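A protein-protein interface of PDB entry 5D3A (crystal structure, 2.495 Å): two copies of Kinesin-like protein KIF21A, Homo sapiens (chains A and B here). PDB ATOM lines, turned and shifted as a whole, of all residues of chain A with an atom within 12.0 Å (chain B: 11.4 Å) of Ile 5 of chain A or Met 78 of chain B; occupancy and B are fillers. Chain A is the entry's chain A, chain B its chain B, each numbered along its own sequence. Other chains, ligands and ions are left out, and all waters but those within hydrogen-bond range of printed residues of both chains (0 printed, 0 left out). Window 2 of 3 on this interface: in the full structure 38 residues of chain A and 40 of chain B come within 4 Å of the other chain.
No position is printed for both chains.
Of the 10 pairs that touch across the chains among the printed residues, none has its exchanged pair printed and touching as well.
Among the printed residues, merely in contact across the chains: Ile 5 of chain A with Met 78 of chain B, Ile 5 of chain A with Glu 79 of chain B, Met 8 of chain A with Asn 74 of chain B, Met 8 of chain A with Ile 75 of chain B, Met 8 of chain A with Met 78 of chain B, Glu 9 of chain A with Ile 75 of chain B, Glu 9 of chain A with Glu 79 of chain B and Met 12 of chain A with Cys 71 of chain B.
Of chain B, only Met 78 (3.6 Å) and Glu 79 (3.5 Å) come within 4 Å of Ile 5 of chain A.
Of the printed residues of chain A, Met 78 of chain B touches Ile 5 and Met 8.
No residue of chain B comes within 4 Å of Gly 1 of chain A.
Ser 2 of chain A touches none of the printed residues of chain B.
No residue of chain B comes within 4 Å of Thr 4 of chain A.
Ser 6 of chain A touches none of the printed residues of chain B.
Asn 7 of chain A touches none of the printed residues of chain B.
Met 8 of chain A touches just these residues of chain B: Cys 71, Asn 74, Ile 75 and Met 78.
Glu 9 of chain A touches just these residues of chain B: Ile 75 (3.7 Å) and Glu 79 (3.6 Å).
Of chain A, only Met 8 comes within 4 Å of Asn 74 of chain B.
Glu 79 of chain B touches just these residues of chain A: Ile 5 (3.5 Å) and Glu 9 (3.6 Å).
No residue of chain A comes within 4 Å of Glu 80 of chain B.
Of the printed residues of chain B, Met 12 of chain A touches Cys 71 and Gln 72.
Of the printed residues of chain A, Gln 72 of chain B touches Met 12 (3.6 Å).
Of the printed residues of chain A, Cys 71 of chain B touches Met 8 (3.2 Å) and Met 12 (3.7 Å).
Ala 73 of chain B touches none of the printed residues of chain A.
The backbone carbonyl oxygen (O) of Met 8 of chain A sits at hydrogen-bond distance from the side-chain sulfur (SG) of Cys 71 of chain B (3.2 Å).
The side-chain amide oxygen (OE1) of Gln 72 of chain B sits close to the side-chain sulfur (SD) of Met 12 of chain A, at 3.6 Å.
O of Asp 70 of chain B lies close to ND2 of Asn 74 of chain B.
O of Met 78 of chain B lies within hydrogen-bond range of NZ of Lys 82 of chain B.
Hydrophobic or aromatic side chains of chain B within 4 Å of the printed part of chain A: Ile 75 and Met 78.
Among the printed residues, 10 pairs touch across the chains.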
ATOM      1  N   GLY A   1     -28.292   9.117  -4.458  1.00  0.00           N
ATOM      2  CA  GLY A   1     -27.396  10.034  -3.695  1.00  0.00           C
ATOM      3  C   GLY A   1     -26.881   9.416  -2.409  1.00  0.00           C
ATOM      4  O   GLY A   1     -25.841   9.822  -1.887  1.00  0.00           O
ATOM      5  N   SER A   2     -27.610   8.430  -1.899  1.00  0.00           N
ATOM      6  CA  SER A   2     -27.233   7.758  -0.660  1.00  0.00           C
ATOM      7  C   SER A   2     -26.329   6.555  -0.920  1.00  0.00           C
ATOM      8  O   SER A   2     -25.942   5.856   0.014  1.00  0.00           O
ATOM      9  CB  SER A   2     -28.482   7.311   0.103  1.00  0.00           C
ATOM     10  OG  SER A   2     -29.181   6.303  -0.606  1.00  0.00           O
ATOM     11  N   MET A   3     -25.995   6.315  -2.186  1.00  0.00           N
ATOM     12  CA  MET A   3     -25.150   5.180  -2.549  1.00  0.00           C
ATOM     13  C   MET A   3     -23.847   5.204  -1.757  1.00  0.00           C
ATOM     14  O   MET A   3     -23.389   4.171  -1.273  1.00  0.00           O
ATOM     15  CB  MET A   3     -24.849   5.186  -4.051  1.00  0.00           C
ATOM     16  CG  MET A   3     -26.068   4.974  -4.942  1.00  0.00           C
ATOM     17  SD  MET A   3     -26.944   3.423  -4.634  1.00  0.00           S
ATOM     18  CE  MET A   3     -25.670   2.215  -4.996  1.00  0.00           C
ATOM     19  N   THR A   4     -23.261   6.388  -1.625  1.00  0.00           N
ATOM     20  CA  THR A   4     -22.004   6.544  -0.905  1.00  0.00           C
ATOM     21  C   THR A   4     -22.255   6.627   0.597  1.00  0.00           C
ATOM     22  O   THR A   4     -21.481   6.099   1.394  1.00  0.00           O
ATOM     23  CB  THR A   4     -21.242   7.800  -1.367  1.00  0.00           C
ATOM     24  OG1 THR A   4     -21.045   7.748  -2.786  1.00  0.00           O
ATOM     25  CG2 THR A   4     -19.891   7.901  -0.672  1.00  0.00           C
ATOM     26  N   ILE A   5     -23.338   7.293   0.980  1.00  0.00           N
ATOM     27  CA  ILE A   5     -23.699   7.402   2.387  1.00  0.00           C
ATOM     28  C   ILE A   5     -24.067   6.018   2.904  1.00  0.00           C
ATOM     29  O   ILE A   5     -23.579   5.583   3.944  1.00  0.00           O
ATOM     30  CB  ILE A   5     -24.850   8.404   2.601  1.00  0.00           C
ATOM     31  CG1 ILE A   5     -24.450   9.786   2.074  1.00  0.00           C
ATOM     32  CG2 ILE A   5     -25.220   8.484   4.080  1.00  0.00           C
ATOM     33  CD1 ILE A   5     -25.585  10.790   2.045  1.00  0.00           C
ATOM     34  N   SER A   6     -24.927   5.328   2.163  1.00  0.00           N
ATOM     35  CA  SER A   6     -25.362   3.988   2.538  1.00  0.00           C
ATOM     36  C   SER A   6     -24.172   3.038   2.600  1.00  0.00           C
ATOM     37  O   SER A   6     -24.134   2.130   3.430  1.00  0.00           O
ATOM     38  CB  SER A   6     -26.405   3.463   1.549  1.00  0.00           C
ATOM     39  OG  SER A   6     -26.878   2.184   1.934  1.00  0.00           O
ATOM     40  N   ASN A   7     -23.203   3.246   1.714  1.00  0.00           N
ATOM     41  CA  ASN A   7     -21.986   2.446   1.722  1.00  0.00           C
ATOM     42  C   ASN A   7     -21.242   2.631   3.039  1.00  0.00           C
ATOM     43  O   ASN A   7     -20.952   1.660   3.736  1.00  0.00           O
ATOM     44  CB  ASN A   7     -21.080   2.821   0.547  1.00  0.00           C
ATOM     45  CG  ASN A   7     -21.429   2.067  -0.723  1.00  0.00           C
ATOM     46  OD1 ASN A   7     -22.485   1.439  -0.817  1.00  0.00           O
ATOM     47  ND2 ASN A   7     -20.541   2.125  -1.709  1.00  0.00           N
ATOM     48  N   MET A   8     -20.943   3.881   3.379  1.00  0.00           N
ATOM     49  CA  MET A   8     -20.238   4.180   4.619  1.00  0.00           C
ATOM     50  C   MET A   8     -20.983   3.591   5.815  1.00  0.00           C
ATOM     51  O   MET A   8     -20.359   3.117   6.765  1.00  0.00           O
ATOM     52  CB  MET A   8     -20.061   5.692   4.788  1.00  0.00           C
ATOM     53  CG  MET A   8     -18.943   6.270   3.928  1.00  0.00           C
ATOM     54  SD  MET A   8     -18.579   8.004   4.267  1.00  0.00           S
ATOM     55  CE  MET A   8     -20.033   8.793   3.588  1.00  0.00           C
ATOM     56  N   GLU A   9     -22.311   3.610   5.764  1.00  0.00           N
ATOM     57  CA  GLU A   9     -23.112   2.971   6.801  1.00  0.00           C
ATOM     58  C   GLU A   9     -22.787   1.485   6.855  1.00  0.00           C
ATOM     59  O   GLU A   9     -22.483   0.943   7.917  1.00  0.00           O
ATOM     60  CB  GLU A   9     -24.610   3.175   6.552  1.00  0.00           C
ATOM     61  CG  GLU A   9     -25.129   4.560   6.926  1.00  0.00           C
ATOM     62  CD  GLU A   9     -26.645   4.665   6.843  1.00  0.00           C
ATOM     63  OE1 GLU A   9     -27.258   3.913   6.055  1.00  0.00           O
ATOM     64  OE2 GLU A   9     -27.224   5.500   7.569  1.00  0.00           O
ATOM     65  N   ALA A  10     -22.853   0.831   5.701  1.00  0.00           N
ATOM     66  CA  ALA A  10     -22.540  -0.588   5.609  1.00  0.00           C
ATOM     67  C   ALA A  10     -21.150  -0.856   6.168  1.00  0.00           C
ATOM     68  O   ALA A  10     -20.944  -1.813   6.912  1.00  0.00           O
ATOM     69  CB  ALA A  10     -22.633  -1.062   4.172  1.00  0.00           C
ATOM     70  N   ASP A  11     -20.196  -0.003   5.805  1.00  0.00           N
ATOM     71  CA  ASP A  11     -18.835  -0.125   6.307  1.00  0.00           C
ATOM     72  C   ASP A  11     -18.829  -0.045   7.827  1.00  0.00           C
ATOM     73  O   ASP A  11     -18.166  -0.836   8.498  1.00  0.00           O
ATOM     74  CB  ASP A  11     -17.937   0.965   5.717  1.00  0.00           C
ATOM     75  CG  ASP A  11     -17.634   0.745   4.245  1.00  0.00           C
ATOM     76  OD1 ASP A  11     -17.719  -0.413   3.780  1.00  0.00           O
ATOM     77  OD2 ASP A  11     -17.302   1.731   3.554  1.00  0.00           O
ATOM     78  N   MET A  12     -19.581   0.909   8.366  1.00  0.00           N
ATOM     79  CA  MET A  12     -19.646   1.105   9.809  1.00  0.00           C
ATOM     80  C   MET A  12     -20.117  -0.157  10.515  1.00  0.00           C
ATOM     81  O   MET A  12     -19.524  -0.574  11.506  1.00  0.00           O
ATOM     82  CB  MET A  12     -20.573   2.268  10.154  1.00  0.00           C
ATOM     83  CG  MET A  12     -20.619   2.594  11.634  1.00  0.00           C
ATOM     84  SD  MET A  12     -21.130   4.293  11.942  1.00  0.00           S
ATOM     85  CE  MET A  12     -21.236   4.288  13.727  1.00  0.00           C
ATOM     86  N   ASN A  13     -21.181  -0.765   9.998  1.00  0.00           N
ATOM     87  CA  ASN A  13     -21.756  -1.954  10.618  1.00  0.00           C
ATOM     88  C   ASN A  13     -20.722  -3.064  10.740  1.00  0.00           C
ATOM     89  O   ASN A  13     -20.693  -3.788  11.732  1.00  0.00           O
ATOM     90  CB  ASN A  13     -22.963  -2.452   9.819  1.00  0.00           C
ATOM     91  CG  ASN A  13     -24.283  -1.995  10.413  1.00  0.00           C
ATOM     92  OD1 ASN A  13     -24.927  -2.729  11.161  1.00  0.00           O
ATOM     93  ND2 ASN A  13     -24.687  -0.772  10.087  1.00  0.00           N
ATOM     94  N   ARG A  14     -19.868  -3.186   9.730  1.00  0.00           N
ATOM     95  CA  ARG A  14     -18.870  -4.249   9.696  1.00  0.00           C
ATOM     96  C   ARG A  14     -17.714  -3.944  10.647  1.00  0.00           C
ATOM     97  O   ARG A  14     -17.102  -4.856  11.201  1.00  0.00           O
ATOM     98  CB  ARG A  14     -18.375  -4.443   8.261  1.00  0.00           C
ATOM     99  CG  ARG A  14     -19.527  -4.714   7.301  1.00  0.00           C
ATOM    100  CD  ARG A  14     -19.093  -4.944   5.865  1.00  0.00           C
ATOM    101  NE  ARG A  14     -20.250  -4.946   4.972  1.00  0.00           N
ATOM    102  CZ  ARG A  14     -21.192  -5.886   4.964  1.00  0.00           C
ATOM    103  NH1 ARG A  14     -21.122  -6.915   5.801  1.00  0.00           N
ATOM    104  NH2 ARG A  14     -22.210  -5.797   4.118  1.00  0.00           N
ATOM    105  N   LEU A  15     -17.428  -2.663  10.841  1.00  0.00           N
ATOM    106  CA  LEU A  15     -16.487  -2.243  11.871  1.00  0.00           C
ATOM    107  C   LEU A  15     -17.045  -2.568  13.251  1.00  0.00           C
ATOM    108  O   LEU A  15     -16.293  -2.883  14.173  1.00  0.00           O
ATOM    109  CB  LEU A  15     -16.194  -0.748  11.769  1.00  0.00           C
ATOM    110  CG  LEU A  15     -15.429  -0.264  10.539  1.00  0.00           C
ATOM    111  CD1 LEU A  15     -15.444   1.254  10.477  1.00  0.00           C
ATOM    112  CD2 LEU A  15     -14.001  -0.780  10.564  1.00  0.00           C
ATOM    113  N   SER B  69     -14.929   5.933  14.486  1.00  0.00           N
ATOM    114  CA  SER B  69     -15.117   7.344  14.804  1.00  0.00           C
ATOM    115  C   SER B  69     -14.940   8.225  13.570  1.00  0.00           C
ATOM    116  O   SER B  69     -15.568   9.278  13.456  1.00  0.00           O
ATOM    117  CB  SER B  69     -14.141   7.775  15.903  1.00  0.00           C
ATOM    118  OG  SER B  69     -14.389   7.074  17.113  1.00  0.00           O
ATOM    119  N   ASP B  70     -14.082   7.795  12.650  1.00  0.00           N
ATOM    120  CA  ASP B  70     -13.878   8.520  11.401  1.00  0.00           C
ATOM    121  C   ASP B  70     -15.033   8.237  10.450  1.00  0.00           C
ATOM    122  O   ASP B  70     -15.487   9.122   9.726  1.00  0.00           O
ATOM    123  CB  ASP B  70     -12.550   8.129  10.751  1.00  0.00           C
ATOM    124  CG  ASP B  70     -11.349   8.692  11.490  1.00  0.00           C
ATOM    125  OD1 ASP B  70     -11.486   9.035  12.685  1.00  0.00           O
ATOM    126  OD2 ASP B  70     -10.264   8.789  10.877  1.00  0.00           O
ATOM    127  N   CYS B  71     -15.504   6.996  10.460  1.00  0.00           N
ATOM    128  CA  CYS B  71     -16.624   6.604   9.619  1.00  0.00           C
ATOM    129  C   CYS B  71     -17.864   7.391  10.017  1.00  0.00           C
ATOM    130  O   CYS B  71     -18.427   8.134   9.216  1.00  0.00           O
ATOM    131  CB  CYS B  71     -16.886   5.103   9.731  1.00  0.00           C
ATOM    132  SG  CYS B  71     -18.115   4.492   8.571  1.00  0.00           S
ATOM    133  N   GLN B  72     -18.278   7.221  11.268  1.00  0.00           N
ATOM    134  CA  GLN B  72     -19.429   7.931  11.813  1.00  0.00           C
ATOM    135  C   GLN B  72     -19.321   9.435  11.581  1.00  0.00           C
ATOM    136  O   GLN B  72     -20.316  10.101  11.302  1.00  0.00           O
ATOM    137  CB  GLN B  72     -19.561   7.637  13.309  1.00  0.00           C
ATOM    138  CG  GLN B  72     -20.545   8.530  14.040  1.00  0.00           C
ATOM    139  CD  GLN B  72     -21.910   8.535  13.395  1.00  0.00           C
ATOM    140  OE1 GLN B  72     -22.332   7.544  12.795  1.00  0.00           O
ATOM    141  NE2 GLN B  72     -22.609   9.656  13.506  1.00  0.00           N
ATOM    142  N   ALA B  73     -18.108   9.964  11.702  1.00  0.00           N
ATOM    143  CA  ALA B  73     -17.873  11.393  11.525  1.00  0.00           C
ATOM    144  C   ALA B  73     -18.188  11.833  10.101  1.00  0.00           C
ATOM    145  O   ALA B  73     -18.867  12.838   9.888  1.00  0.00           O
ATOM    146  CB  ALA B  73     -16.438  11.735  11.872  1.00  0.00           C
ATOM    147  N   ASN B  74     -17.687  11.078   9.129  1.00  0.00           N
ATOM    148  CA  ASN B  74     -17.896  11.399   7.724  1.00  0.00           C
ATOM    149  C   ASN B  74     -19.366  11.255   7.350  1.00  0.00           C
ATOM    150  O   ASN B  74     -19.907  12.072   6.606  1.00  0.00           O
ATOM    151  CB  ASN B  74     -17.034  10.500   6.836  1.00  0.00           C
ATOM    152  CG  ASN B  74     -15.553  10.626   7.143  1.00  0.00           C
ATOM    153  OD1 ASN B  74     -15.107  11.610   7.739  1.00  0.00           O
ATOM    154  ND2 ASN B  74     -14.779   9.628   6.734  1.00  0.00           N
ATOM    155  N   ILE B  75     -20.005  10.209   7.864  1.00  0.00           N
ATOM    156  CA  ILE B  75     -21.431  10.003   7.649  1.00  0.00           C
ATOM    157  C   ILE B  75     -22.182  11.249   8.094  1.00  0.00           C
ATOM    158  O   ILE B  75     -23.081  11.727   7.405  1.00  0.00           O
ATOM    159  CB  ILE B  75     -21.932   8.746   8.393  1.00  0.00           C
ATOM    160  CG1 ILE B  75     -21.337   7.490   7.744  1.00  0.00           C
ATOM    161  CG2 ILE B  75     -23.461   8.696   8.394  1.00  0.00           C
ATOM    162  CD1 ILE B  75     -21.724   6.173   8.411  1.00  0.00           C
ATOM    163  N   MET B  76     -21.793  11.774   9.250  1.00  0.00           N
ATOM    164  CA  MET B  76     -22.437  12.945   9.828  1.00  0.00           C
ATOM    165  C   MET B  76     -22.375  14.137   8.874  1.00  0.00           C
ATOM    166  O   MET B  76     -23.408  14.692   8.495  1.00  0.00           O
ATOM    167  CB  MET B  76     -21.773  13.294  11.158  1.00  0.00           C
ATOM    168  CG  MET B  76     -22.632  14.112  12.095  1.00  0.00           C
ATOM    169  SD  MET B  76     -22.007  14.023  13.785  1.00  0.00           S
ATOM    170  CE  MET B  76     -23.251  14.978  14.651  1.00  0.00           C
ATOM    171  N   GLN B  77     -21.160  14.518   8.489  1.00  0.00           N
ATOM    172  CA  GLN B  77     -20.945  15.644   7.581  1.00  0.00           C
ATOM    173  C   GLN B  77     -21.849  15.572   6.354  1.00  0.00           C
ATOM    174  O   GLN B  77     -22.423  16.577   5.938  1.00  0.00           O
ATOM    175  CB  GLN B  77     -19.485  15.699   7.130  1.00  0.00           C
ATOM    176  CG  GLN B  77     -18.488  15.901   8.258  1.00  0.00           C
ATOM    177  CD  GLN B  77     -17.061  16.016   7.753  1.00  0.00           C
ATOM    178  OE1 GLN B  77     -16.801  16.651   6.729  1.00  0.00           O
ATOM    179  NE2 GLN B  77     -16.128  15.392   8.466  1.00  0.00           N
ATOM    180  N   MET B  78     -21.965  14.383   5.772  1.00  0.00           N
ATOM    181  CA  MET B  78     -22.802  14.199   4.597  1.00  0.00           C
ATOM    182  C   MET B  78     -24.279  14.336   4.946  1.00  0.00           C
ATOM    183  O   MET B  78     -25.058  14.880   4.165  1.00  0.00           O
ATOM    184  CB  MET B  78     -22.548  12.833   3.957  1.00  0.00           C
ATOM    185  CG  MET B  78     -21.229  12.725   3.206  1.00  0.00           C
ATOM    186  SD  MET B  78     -21.264  11.419   1.960  1.00  0.00           S
ATOM    187  CE  MET B  78     -19.599  11.521   1.313  1.00  0.00           C
ATOM    188  N   GLU B  79     -24.661  13.844   6.120  1.00  0.00           N
ATOM    189  CA  GLU B  79     -26.068  13.801   6.503  1.00  0.00           C
ATOM    190  C   GLU B  79     -26.516  15.070   7.219  1.00  0.00           C
ATOM    191  O   GLU B  79     -27.687  15.445   7.156  1.00  0.00           O
ATOM    192  CB  GLU B  79     -26.339  12.589   7.395  1.00  0.00           C
ATOM    193  CG  GLU B  79     -26.216  11.256   6.680  1.00  0.00           C
ATOM    194  CD  GLU B  79     -26.539  10.079   7.579  1.00  0.00           C
ATOM    195  OE1 GLU B  79     -26.386  10.205   8.813  1.00  0.00           O
ATOM    196  OE2 GLU B  79     -26.947   9.024   7.050  1.00  0.00           O
ATOM    197  N   GLU B  80     -25.588  15.735   7.897  1.00  0.00           N
ATOM    198  CA  GLU B  80     -25.947  16.899   8.696  1.00  0.00           C
ATOM    199  C   GLU B  80     -26.543  18.003   7.825  1.00  0.00           C
ATOM    200  O   GLU B  80     -26.339  18.037   6.610  1.00  0.00           O
ATOM    201  CB  GLU B  80     -24.732  17.427   9.462  1.00  0.00           C
ATOM    202  CG  GLU B  80     -23.636  18.015   8.595  1.00  0.00           C
ATOM    203  CD  GLU B  80     -22.503  18.597   9.415  1.00  0.00           C
ATOM    204  OE1 GLU B  80     -22.526  18.448  10.656  1.00  0.00           O
ATOM    205  OE2 GLU B  80     -21.591  19.204   8.819  1.00  0.00           O
ATOM    206  N   ALA B  81     -27.292  18.897   8.462  1.00  0.00           N
ATOM    207  CA  ALA B  81     -27.891  20.033   7.777  1.00  0.00           C
ATOM    208  C   ALA B  81     -26.813  20.913   7.148  1.00  0.00           C
ATOM    209  O   ALA B  81     -25.709  21.041   7.682  1.00  0.00           O
ATOM    210  CB  ALA B  81     -28.742  20.845   8.747  1.00  0.00           C
ATOM    211  N   LYS B  82     -27.141  21.514   6.010  1.00  0.00           N
ATOM    212  CA  LYS B  82     -26.209  22.390   5.309  1.00  0.00           C
ATOM    213  C   LYS B  82     -26.959  23.530   4.632  1.00  0.00           C
ATOM    214  O   LYS B  82     -26.407  24.611   4.420  1.00  0.00           O
ATOM    215  CB  LYS B  82     -25.398  21.601   4.277  1.00  0.00           C
ATOM    216  CG  LYS B  82     -24.358  20.666   4.891  1.00  0.00           C
ATOM    217  CD  LYS B  82     -23.718  19.747   3.855  1.00  0.00           C
ATOM    218  CE  LYS B  82     -24.685  18.680   3.357  1.00  0.00           C
ATOM    219  NZ  LYS B  82     -25.219  17.830   4.462  1.00  0.00           N
ATOM    220  OXT LYS B  82     -28.133  23.400   4.286  1.00  0.00           O
